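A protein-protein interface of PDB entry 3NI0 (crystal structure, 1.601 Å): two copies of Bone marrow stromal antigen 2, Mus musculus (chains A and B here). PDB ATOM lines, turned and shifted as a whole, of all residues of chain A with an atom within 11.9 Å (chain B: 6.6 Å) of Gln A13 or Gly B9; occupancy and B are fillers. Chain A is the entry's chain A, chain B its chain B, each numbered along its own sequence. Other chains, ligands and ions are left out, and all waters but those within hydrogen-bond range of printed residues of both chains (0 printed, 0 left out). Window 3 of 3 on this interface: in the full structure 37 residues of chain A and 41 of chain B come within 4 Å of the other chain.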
ATOM      1  N   ALA A   5      25.277 -11.886   0.850  1.00  0.00           N
ATOM      2  CA  ALA A   5      24.960 -12.984   1.754  1.00  0.00           C
ATOM      3  C   ALA A   5      24.006 -12.510   2.849  1.00  0.00           C
ATOM      4  O   ALA A   5      23.074 -11.752   2.579  1.00  0.00           O
ATOM      5  CB  ALA A   5      26.237 -13.552   2.358  1.00  0.00           C
ATOM      6  N   CYS A   6      24.234 -12.957   4.080  1.00  0.00           N
ATOM      7  CA  CYS A   6      23.415 -12.526   5.208  1.00  0.00           C
ATOM      8  C   CYS A   6      23.938 -11.222   5.802  1.00  0.00           C
ATOM      9  O   CYS A   6      23.489 -10.792   6.864  1.00  0.00           O
ATOM     10  CB  CYS A   6      23.359 -13.611   6.287  1.00  0.00           C
ATOM     11  SG  CYS A   6      22.200 -14.960   5.938  1.00  0.00           S
ATOM     12  N   ARG A   7      24.892 -10.598   5.117  1.00  0.00           N
ATOM     13  CA  ARG A   7      25.395  -9.295   5.533  1.00  0.00           C
ATOM     14  C   ARG A   7      24.255  -8.288   5.542  1.00  0.00           C
ATOM     15  O   ARG A   7      24.150  -7.460   6.447  1.00  0.00           O
ATOM     16  CB  ARG A   7      26.493  -8.809   4.588  1.00  0.00           C
ATOM     17  CG  ARG A   7      27.719  -9.697   4.541  1.00  0.00           C
ATOM     18  CD  ARG A   7      28.852  -9.013   3.795  1.00  0.00           C
ATOM     19  NE  ARG A   7      30.052  -9.845   3.734  1.00  0.00           N
ATOM     20  CZ  ARG A   7      30.454 -10.512   2.655  1.00  0.00           C
ATOM     21  NH1 ARG A   7      29.770 -10.440   1.519  1.00  0.00           N
ATOM     22  NH2 ARG A   7      31.559 -11.244   2.709  1.00  0.00           N
ATOM     23  N   ASP A   8      23.406  -8.359   4.522  1.00  0.00           N
ATOM     24  CA  ASP A   8      22.269  -7.455   4.404  1.00  0.00           C
ATOM     25  C   ASP A   8      21.351  -7.579   5.614  1.00  0.00           C
ATOM     26  O   ASP A   8      20.792  -6.590   6.085  1.00  0.00           O
ATOM     27  CB  ASP A   8      21.489  -7.750   3.120  1.00  0.00           C
ATOM     28  CG  ASP A   8      22.297  -7.465   1.868  1.00  0.00           C
ATOM     29  OD1 ASP A   8      22.231  -6.324   1.365  1.00  0.00           O
ATOM     30  OD2 ASP A   8      22.996  -8.380   1.386  1.00  0.00           O
ATOM     31  N   GLY A   9      21.196  -8.802   6.110  1.00  0.00           N
ATOM     32  CA  GLY A   9      20.352  -9.057   7.264  1.00  0.00           C
ATOM     33  C   GLY A   9      20.907  -8.450   8.539  1.00  0.00           C
ATOM     34  O   GLY A   9      20.173  -7.831   9.308  1.00  0.00           O
ATOM     35  N   LEU A  10      22.205  -8.628   8.766  1.00  0.00           N
ATOM     36  CA  LEU A  10      22.859  -8.071   9.944  1.00  0.00           C
ATOM     37  C   LEU A  10      22.725  -6.553   9.967  1.00  0.00           C
ATOM     38  O   LEU A  10      22.505  -5.954  11.019  1.00  0.00           O
ATOM     39  CB  LEU A  10      24.342  -8.454   9.970  1.00  0.00           C
ATOM     40  CG  LEU A  10      24.684  -9.864  10.454  1.00  0.00           C
ATOM     41  CD1 LEU A  10      26.161 -10.148  10.241  1.00  0.00           C
ATOM     42  CD2 LEU A  10      24.309 -10.038  11.919  1.00  0.00           C
ATOM     43  N   ARG A  11      22.864  -5.935   8.800  1.00  0.00           N
ATOM     44  CA  ARG A  11      22.768  -4.486   8.687  1.00  0.00           C
ATOM     45  C   ARG A  11      21.361  -3.995   8.997  1.00  0.00           C
ATOM     46  O   ARG A  11      21.187  -2.970   9.652  1.00  0.00           O
ATOM     47  CB  ARG A  11      23.171  -4.035   7.287  1.00  0.00           C
ATOM     48  CG  ARG A  11      24.649  -4.187   7.013  1.00  0.00           C
ATOM     49  CD  ARG A  11      25.011  -3.671   5.638  1.00  0.00           C
ATOM     50  NE  ARG A  11      26.456  -3.557   5.491  1.00  0.00           N
ATOM     51  CZ  ARG A  11      27.226  -4.444   4.871  1.00  0.00           C
ATOM     52  NH1 ARG A  11      26.704  -5.531   4.316  1.00  0.00           N
ATOM     53  NH2 ARG A  11      28.531  -4.242   4.809  1.00  0.00           N
ATOM     54  N   ALA A  12      20.360  -4.727   8.520  1.00  0.00           N
ATOM     55  CA  ALA A  12      18.970  -4.362   8.762  1.00  0.00           C
ATOM     56  C   ALA A  12      18.646  -4.466  10.246  1.00  0.00           C
ATOM     57  O   ALA A  12      17.930  -3.628  10.794  1.00  0.00           O
ATOM     58  CB  ALA A  12      18.042  -5.254   7.955  1.00  0.00           C
ATOM     59  N   GLN A  13      19.180  -5.497  10.889  1.00  0.00           N
ATOM     60  CA  GLN A  13      18.923  -5.740  12.303  1.00  0.00           C
ATOM     61  C   GLN A  13      19.567  -4.657  13.161  1.00  0.00           C
ATOM     62  O   GLN A  13      19.007  -4.240  14.173  1.00  0.00           O
ATOM     63  CB  GLN A  13      19.460  -7.111  12.715  1.00  0.00           C
ATOM     64  CG  GLN A  13      18.910  -7.616  14.038  1.00  0.00           C
ATOM     65  CD  GLN A  13      17.449  -8.004  13.945  1.00  0.00           C
ATOM     66  OE1 GLN A  13      17.047  -8.746  13.048  1.00  0.00           O
ATOM     67  NE2 GLN A  13      16.640  -7.493  14.867  1.00  0.00           N
ATOM     68  N   ALA A  14      20.751  -4.207  12.752  1.00  0.00           N
ATOM     69  CA  ALA A  14      21.455  -3.151  13.470  1.00  0.00           C
ATOM     70  C   ALA A  14      20.687  -1.844  13.350  1.00  0.00           C
ATOM     71  O   ALA A  14      20.517  -1.122  14.332  1.00  0.00           O
ATOM     72  CB  ALA A  14      22.860  -2.987  12.923  1.00  0.00           C
ATOM     73  N   GLU A  15      20.225  -1.548  12.141  1.00  0.00           N
ATOM     74  CA  GLU A  15      19.456  -0.340  11.887  1.00  0.00           C
ATOM     75  C   GLU A  15      18.222  -0.304  12.779  1.00  0.00           C
ATOM     76  O   GLU A  15      17.921   0.718  13.385  1.00  0.00           O
ATOM     77  CB  GLU A  15      19.047  -0.265  10.413  1.00  0.00           C
ATOM     78  CG  GLU A  15      18.182   0.939  10.065  1.00  0.00           C
ATOM     79  CD  GLU A  15      17.976   1.090   8.572  1.00  0.00           C
ATOM     80  OE1 GLU A  15      18.470   0.230   7.814  1.00  0.00           O
ATOM     81  OE2 GLU A  15      17.327   2.070   8.152  1.00  0.00           O
ATOM     82  N   CYS A  16      17.514  -1.425  12.868  1.00  0.00           N
ATOM     83  CA  CYS A  16      16.284  -1.476  13.648  1.00  0.00           C
ATOM     84  C   CYS A  16      16.573  -1.332  15.139  1.00  0.00           C
ATOM     85  O   CYS A  16      15.830  -0.664  15.858  1.00  0.00           O
ATOM     86  CB  CYS A  16      15.529  -2.778  13.380  1.00  0.00           C
ATOM     87  SG  CYS A  16      13.819  -2.758  13.971  1.00  0.00           S
ATOM     88  N   ARG A  17      17.653  -1.955  15.599  1.00  0.00           N
ATOM     89  CA  ARG A  17      18.048  -1.865  17.002  1.00  0.00           C
ATOM     90  C   ARG A  17      18.409  -0.428  17.363  1.00  0.00           C
ATOM     91  O   ARG A  17      18.052   0.065  18.432  1.00  0.00           O
ATOM     92  CB  ARG A  17      19.245  -2.770  17.292  1.00  0.00           C
ATOM     93  CG  ARG A  17      19.473  -3.002  18.776  1.00  0.00           C
ATOM     94  CD  ARG A  17      20.948  -2.965  19.148  1.00  0.00           C
ATOM     95  NE  ARG A  17      21.138  -3.127  20.588  1.00  0.00           N
ATOM     96  CZ  ARG A  17      20.851  -2.194  21.491  1.00  0.00           C
ATOM     97  NH1 ARG A  17      20.354  -1.024  21.109  1.00  0.00           N
ATOM     98  NH2 ARG A  17      21.056  -2.431  22.780  1.00  0.00           N
ATOM     99  N   ASN A  18      19.123   0.238  16.462  1.00  0.00           N
ATOM    100  CA  ASN A  18      19.525   1.623  16.669  1.00  0.00           C
ATOM    101  C   ASN A  18      18.319   2.541  16.690  1.00  0.00           C
ATOM    102  O   ASN A  18      18.266   3.490  17.468  1.00  0.00           O
ATOM    103  CB  ASN A  18      20.472   2.081  15.562  1.00  0.00           C
ATOM    104  CG  ASN A  18      21.792   1.345  15.584  1.00  0.00           C
ATOM    105  OD1 ASN A  18      22.188   0.781  16.602  1.00  0.00           O
ATOM    106  ND2 ASN A  18      22.488   1.355  14.457  1.00  0.00           N
ATOM    107  N   THR A  19      17.353   2.252  15.827  1.00  0.00           N
ATOM    108  CA  THR A  19      16.172   3.093  15.694  1.00  0.00           C
ATOM    109  C   THR A  19      15.309   3.003  16.947  1.00  0.00           C
ATOM    110  O   THR A  19      14.835   4.018  17.444  1.00  0.00           O
ATOM    111  CB  THR A  19      15.332   2.701  14.466  1.00  0.00           C
ATOM    112  OG1 THR A  19      16.117   2.839  13.278  1.00  0.00           O
ATOM    113  CG2 THR A  19      14.105   3.592  14.351  1.00  0.00           C
ATOM    114  N   THR A  20      15.106   1.791  17.455  1.00  0.00           N
ATOM    115  CA  THR A  20      14.338   1.604  18.684  1.00  0.00           C
ATOM    116  C   THR A  20      15.044   2.282  19.853  1.00  0.00           C
ATOM    117  O   THR A  20      14.405   2.909  20.699  1.00  0.00           O
ATOM    118  CB  THR A  20      14.141   0.115  19.025  1.00  0.00           C
ATOM    119  OG1 THR A  20      15.417  -0.520  19.149  1.00  0.00           O
ATOM    120  CG2 THR A  20      13.323  -0.587  17.951  1.00  0.00           C
ATOM    121  N   HIS A  21      16.365   2.150  19.889  1.00  0.00           N
ATOM    122  CA  HIS A  21      17.182   2.741  20.939  1.00  0.00           C
ATOM    123  C   HIS A  21      16.972   4.251  20.968  1.00  0.00           C
ATOM    124  O   HIS A  21      16.729   4.841  22.023  1.00  0.00           O
ATOM    125  CB  HIS A  21      18.657   2.412  20.682  1.00  0.00           C
ATOM    126  CG  HIS A  21      19.581   2.834  21.789  1.00  0.00           C
ATOM    127  ND1 HIS A  21      20.087   4.112  21.882  1.00  0.00           N
ATOM    128  CD2 HIS A  21      20.091   2.144  22.826  1.00  0.00           C
ATOM    129  CE1 HIS A  21      20.869   4.192  22.944  1.00  0.00           C
ATOM    130  NE2 HIS A  21      20.891   3.011  23.540  1.00  0.00           N
ATOM    131  N   LEU A  22      17.049   4.864  19.793  1.00  0.00           N
ATOM    132  CA  LEU A  22      16.898   6.304  19.651  1.00  0.00           C
ATOM    133  C   LEU A  22      15.485   6.750  20.008  1.00  0.00           C
ATOM    134  O   LEU A  22      15.301   7.761  20.681  1.00  0.00           O
ATOM    135  CB  LEU A  22      17.220   6.730  18.219  1.00  0.00           C
ATOM    136  CG  LEU A  22      17.040   8.221  17.930  1.00  0.00           C
ATOM    137  CD1 LEU A  22      17.850   9.056  18.913  1.00  0.00           C
ATOM    138  CD2 LEU A  22      17.428   8.543  16.497  1.00  0.00           C
ATOM    139  N   CYS B   6      18.018 -16.436   5.630  1.00  0.00           N
ATOM    140  CA  CYS B   6      18.046 -16.841   7.029  1.00  0.00           C
ATOM    141  C   CYS B   6      16.656 -16.713   7.644  1.00  0.00           C
ATOM    142  O   CYS B   6      15.770 -16.079   7.070  1.00  0.00           O
ATOM    143  CB  CYS B   6      19.038 -15.979   7.813  1.00  0.00           C
ATOM    144  SG  CYS B   6      20.625 -15.714   6.979  1.00  0.00           S
ATOM    145  N   ARG B   7      16.471 -17.325   8.808  1.00  0.00           N
ATOM    146  CA  ARG B   7      15.223 -17.205   9.552  1.00  0.00           C
ATOM    147  C   ARG B   7      15.494 -16.558  10.903  1.00  0.00           C
ATOM    148  O   ARG B   7      14.654 -15.837  11.440  1.00  0.00           O
ATOM    149  CB  ARG B   7      14.588 -18.578   9.762  1.00  0.00           C
ATOM    150  CG  ARG B   7      14.480 -19.425   8.507  1.00  0.00           C
ATOM    151  CD  ARG B   7      13.838 -20.764   8.824  1.00  0.00           C
ATOM    152  NE  ARG B   7      13.830 -21.670   7.679  1.00  0.00           N
ATOM    153  CZ  ARG B   7      13.238 -22.860   7.677  1.00  0.00           C
ATOM    154  NH1 ARG B   7      12.600 -23.290   8.758  1.00  0.00           N
ATOM    155  NH2 ARG B   7      13.281 -23.621   6.593  1.00  0.00           N
ATOM    156  N   ASP B   8      16.673 -16.835  11.451  1.00  0.00           N
ATOM    157  CA  ASP B   8      17.106 -16.234  12.705  1.00  0.00           C
ATOM    158  C   ASP B   8      16.936 -14.720  12.665  1.00  0.00           C
ATOM    159  O   ASP B   8      16.730 -14.079  13.696  1.00  0.00           O
ATOM    160  CB  ASP B   8      18.570 -16.588  12.977  1.00  0.00           C
ATOM    161  CG  ASP B   8      19.475 -16.288  11.794  1.00  0.00           C
ATOM    162  OD1 ASP B   8      20.248 -17.185  11.393  1.00  0.00           O
ATOM    163  OD2 ASP B   8      19.423 -15.157  11.268  1.00  0.00           O
ATOM    164  N   GLY B   9      17.021 -14.155  11.465  1.00  0.00           N
ATOM    165  CA  GLY B   9      16.910 -12.720  11.286  1.00  0.00           C
ATOM    166  C   GLY B   9      15.489 -12.275  11.005  1.00  0.00           C
ATOM    167  O   GLY B   9      15.066 -11.223  11.472  1.00  0.00           O
ATOM    168  N   LEU B  10      14.753 -13.075  10.240  1.00  0.00           N
ATOM    169  CA  LEU B  10      13.390 -12.725   9.852  1.00  0.00           C
ATOM    170  C   LEU B  10      12.501 -12.525  11.077  1.00  0.00           C
ATOM    171  O   LEU B  10      11.724 -11.573  11.137  1.00  0.00           O
ATOM    172  CB  LEU B  10      12.803 -13.802   8.937  1.00  0.00           C
ATOM    173  CG  LEU B  10      11.551 -13.418   8.139  1.00  0.00           C
ATOM    174  CD1 LEU B  10      11.381 -14.347   6.947  1.00  0.00           C
ATOM    175  CD2 LEU B  10      10.302 -13.427   9.009  1.00  0.00           C
ATOM    176  N   ARG B  11      12.614 -13.422  12.051  1.00  0.00           N
ATOM    177  CA  ARG B  11      11.838 -13.307  13.280  1.00  0.00           C
ATOM    178  C   ARG B  11      12.278 -12.081  14.069  1.00  0.00           C
ATOM    179  O   ARG B  11      11.451 -11.266  14.478  1.00  0.00           O
ATOM    180  CB  ARG B  11      11.997 -14.560  14.142  1.00  0.00           C
ATOM    181  CG  ARG B  11      11.240 -14.497  15.463  1.00  0.00           C
ATOM    182  CD  ARG B  11       9.770 -14.176  15.243  1.00  0.00           C
ATOM    183  NE  ARG B  11       9.114 -15.170  14.397  1.00  0.00           N
ATOM    184  CZ  ARG B  11       8.283 -16.111  14.840  1.00  0.00           C
ATOM    185  NH1 ARG B  11       7.983 -16.196  16.130  1.00  0.00           N
ATOM    186  NH2 ARG B  11       7.742 -16.967  13.984  1.00  0.00           N
ATOM    187  N   ALA B  12      13.585 -11.959  14.281  1.00  0.00           N
ATOM    188  CA  ALA B  12      14.146 -10.834  15.017  1.00  0.00           C
ATOM    189  C   ALA B  12      13.787  -9.504  14.358  1.00  0.00           C
ATOM    190  O   ALA B  12      13.675  -8.483  15.033  1.00  0.00           O
ATOM    191  CB  ALA B  12      15.654 -10.979  15.122  1.00  0.00           C
ATOM    192  N   GLN B  13      13.594  -9.523  13.043  1.00  0.00           N
ATOM    193  CA  GLN B  13      13.320  -8.301  12.292  1.00  0.00           C
ATOM    194  C   GLN B  13      11.863  -7.886  12.419  1.00  0.00           C
ATOM    195  O   GLN B  13      11.564  -6.714  12.635  1.00  0.00           O
ATOM    196  CB  GLN B  13      13.673  -8.478  10.812  1.00  0.00           C
ATOM    197  CG  GLN B  13      14.995  -7.844  10.393  1.00  0.00           C
ATOM    198  CD  GLN B  13      15.139  -6.410  10.872  1.00  0.00           C
ATOM    199  OE1 GLN B  13      14.886  -5.464  10.126  1.00  0.00           O
ATOM    200  NE2 GLN B  13      15.549  -6.243  12.124  1.00  0.00           N
ATOM    201  N   ALA B  14      10.960  -8.850  12.280  1.00  0.00           N
ATOM    202  CA  ALA B  14       9.534  -8.581  12.388  1.00  0.00           C
ATOM    203  C   ALA B  14       9.206  -8.050  13.778  1.00  0.00           C
ATOM    204  O   ALA B  14       8.377  -7.153  13.930  1.00  0.00           O
ATOM    205  CB  ALA B  14       8.738  -9.839  12.099  1.00  0.00           C
ATOM    206  N   CYS B  16      11.410  -6.486  15.891  1.00  0.00           N
ATOM    207  CA  CYS B  16      12.005  -5.161  16.009  1.00  0.00           C
ATOM    208  C   CYS B  16      11.190  -4.128  15.234  1.00  0.00           C
ATOM    209  O   CYS B  16      11.190  -2.947  15.575  1.00  0.00           O
ATOM    210  CB  CYS B  16      13.452  -5.178  15.511  1.00  0.00           C
ATOM    211  SG  CYS B  16      14.333  -3.615  15.737  1.00  0.00           S
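The side-chain sulfur (SG) of Cys A6 forms a disulfide with the side-chain sulfur (SG) of Cys B6, 2.0 Å away.
NE2 of Gln A13 lies within hydrogen-bond range of O of Ala B12, 3.1 Å away.
The side-chain amide oxygen (OE1) of Gln A13 sits at hydrogen-bond distance from the side-chain amide nitrogen (NE2) of Gln B13 (3.1 Å).
The side-chain sulfur (SG) of Cys B16 forms a disulfide with the side-chain sulfur (SG) of Cys A16, 2.0 Å away.
SG of Cys B16 sits at hydrogen-bond distance from N of Arg A17 (3.7 Å).
The backbone carbonyl oxygen (O) of Cys A16 lies close to the side-chain hydroxyl (OG1) of Thr A20, at 3.3 Å.
The backbone carbonyl oxygen of Arg A17 is in hydrogen-bond range of the side-chain hydroxyl of Thr A20, at 2.8 Å.
Among the printed residues, merely in contact across the chains: Ala A12 with Gln B13, Gln A13 with Gly B9, Gln A13 with Cys B16, Cys A16 with Gln B13 and Thr A20 with Cys B16.
Of the printed residues of chain B, Cys A6 touches Cys B6 (2.0 Å).
Of the printed residues of chain B, Gln A13 touches Gly B9 (3.5 Å), Ala B12 (3.1 Å), Gln B13 (3.1 Å) and Cys B16 (3.99 Å).
Of the printed residues of chain B, Cys A16 touches Gln B13 (3.7 Å) and Cys B16 (2.0 Å).
Printed residues of chain B within 4 Å of Arg A17: Cys B16 (3.7 Å).
Of the printed residues of chain B, Thr A20 touches Cys B16.
Of the printed residues of chain A, Cys B6 touches Cys A6 (2.0 Å).
No residue of chain A comes within 4 Å of Asp B8.
Of the printed residues of chain A, Gly B9 touches Gln A13 (3.5 Å).
Of chain A, only Gln A13 (3.1 Å) comes within 4 Å of Ala B12.
Printed residues of chain A within 4 Å of Gln B13: Ala A12, Gln A13 and Cys A16.
Of the printed residues of chain A, Cys B16 touches Gln A13 (3.99 Å), Cys A16 (2.0 Å), Arg A17 (3.7 Å) and Thr A20 (3.9 Å).
The nearest printed residue of chain B that does not touch Gln A13 is Asp B8 (5.4 Å).
The nearest residue of chain A that does not touch Gly B9 is Gly A9 (6.2 Å).
Printed residues of chain B that touch a printed residue of chain A: Cys B6, Gly B9, Ala B12, Gln B13 and Cys B16.
Hydrophobic or aromatic side chains of chain B that line the printed part of chain A: Ala B12.
Along chain B the printed residues that touch a printed residue of chain A span positions 6 to 16.
Among the printed residues, no Asp or Glu carboxylate lies within 4 Å of a Lys or Arg side-chain nitrogen of the other chain.
Cys B6 touches its own counterpart, Cys A6.
Gln A13 touches Gly B9, but with the chains exchanged Gly A9 does not touch Gln B13 (5.3 Å).
Gln A13 touches Cys B16, and with the chains exchanged Cys A16 touches Gln B13.
Cys A16 touches its own counterpart, Cys B16.
10 positions are printed for both chains.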
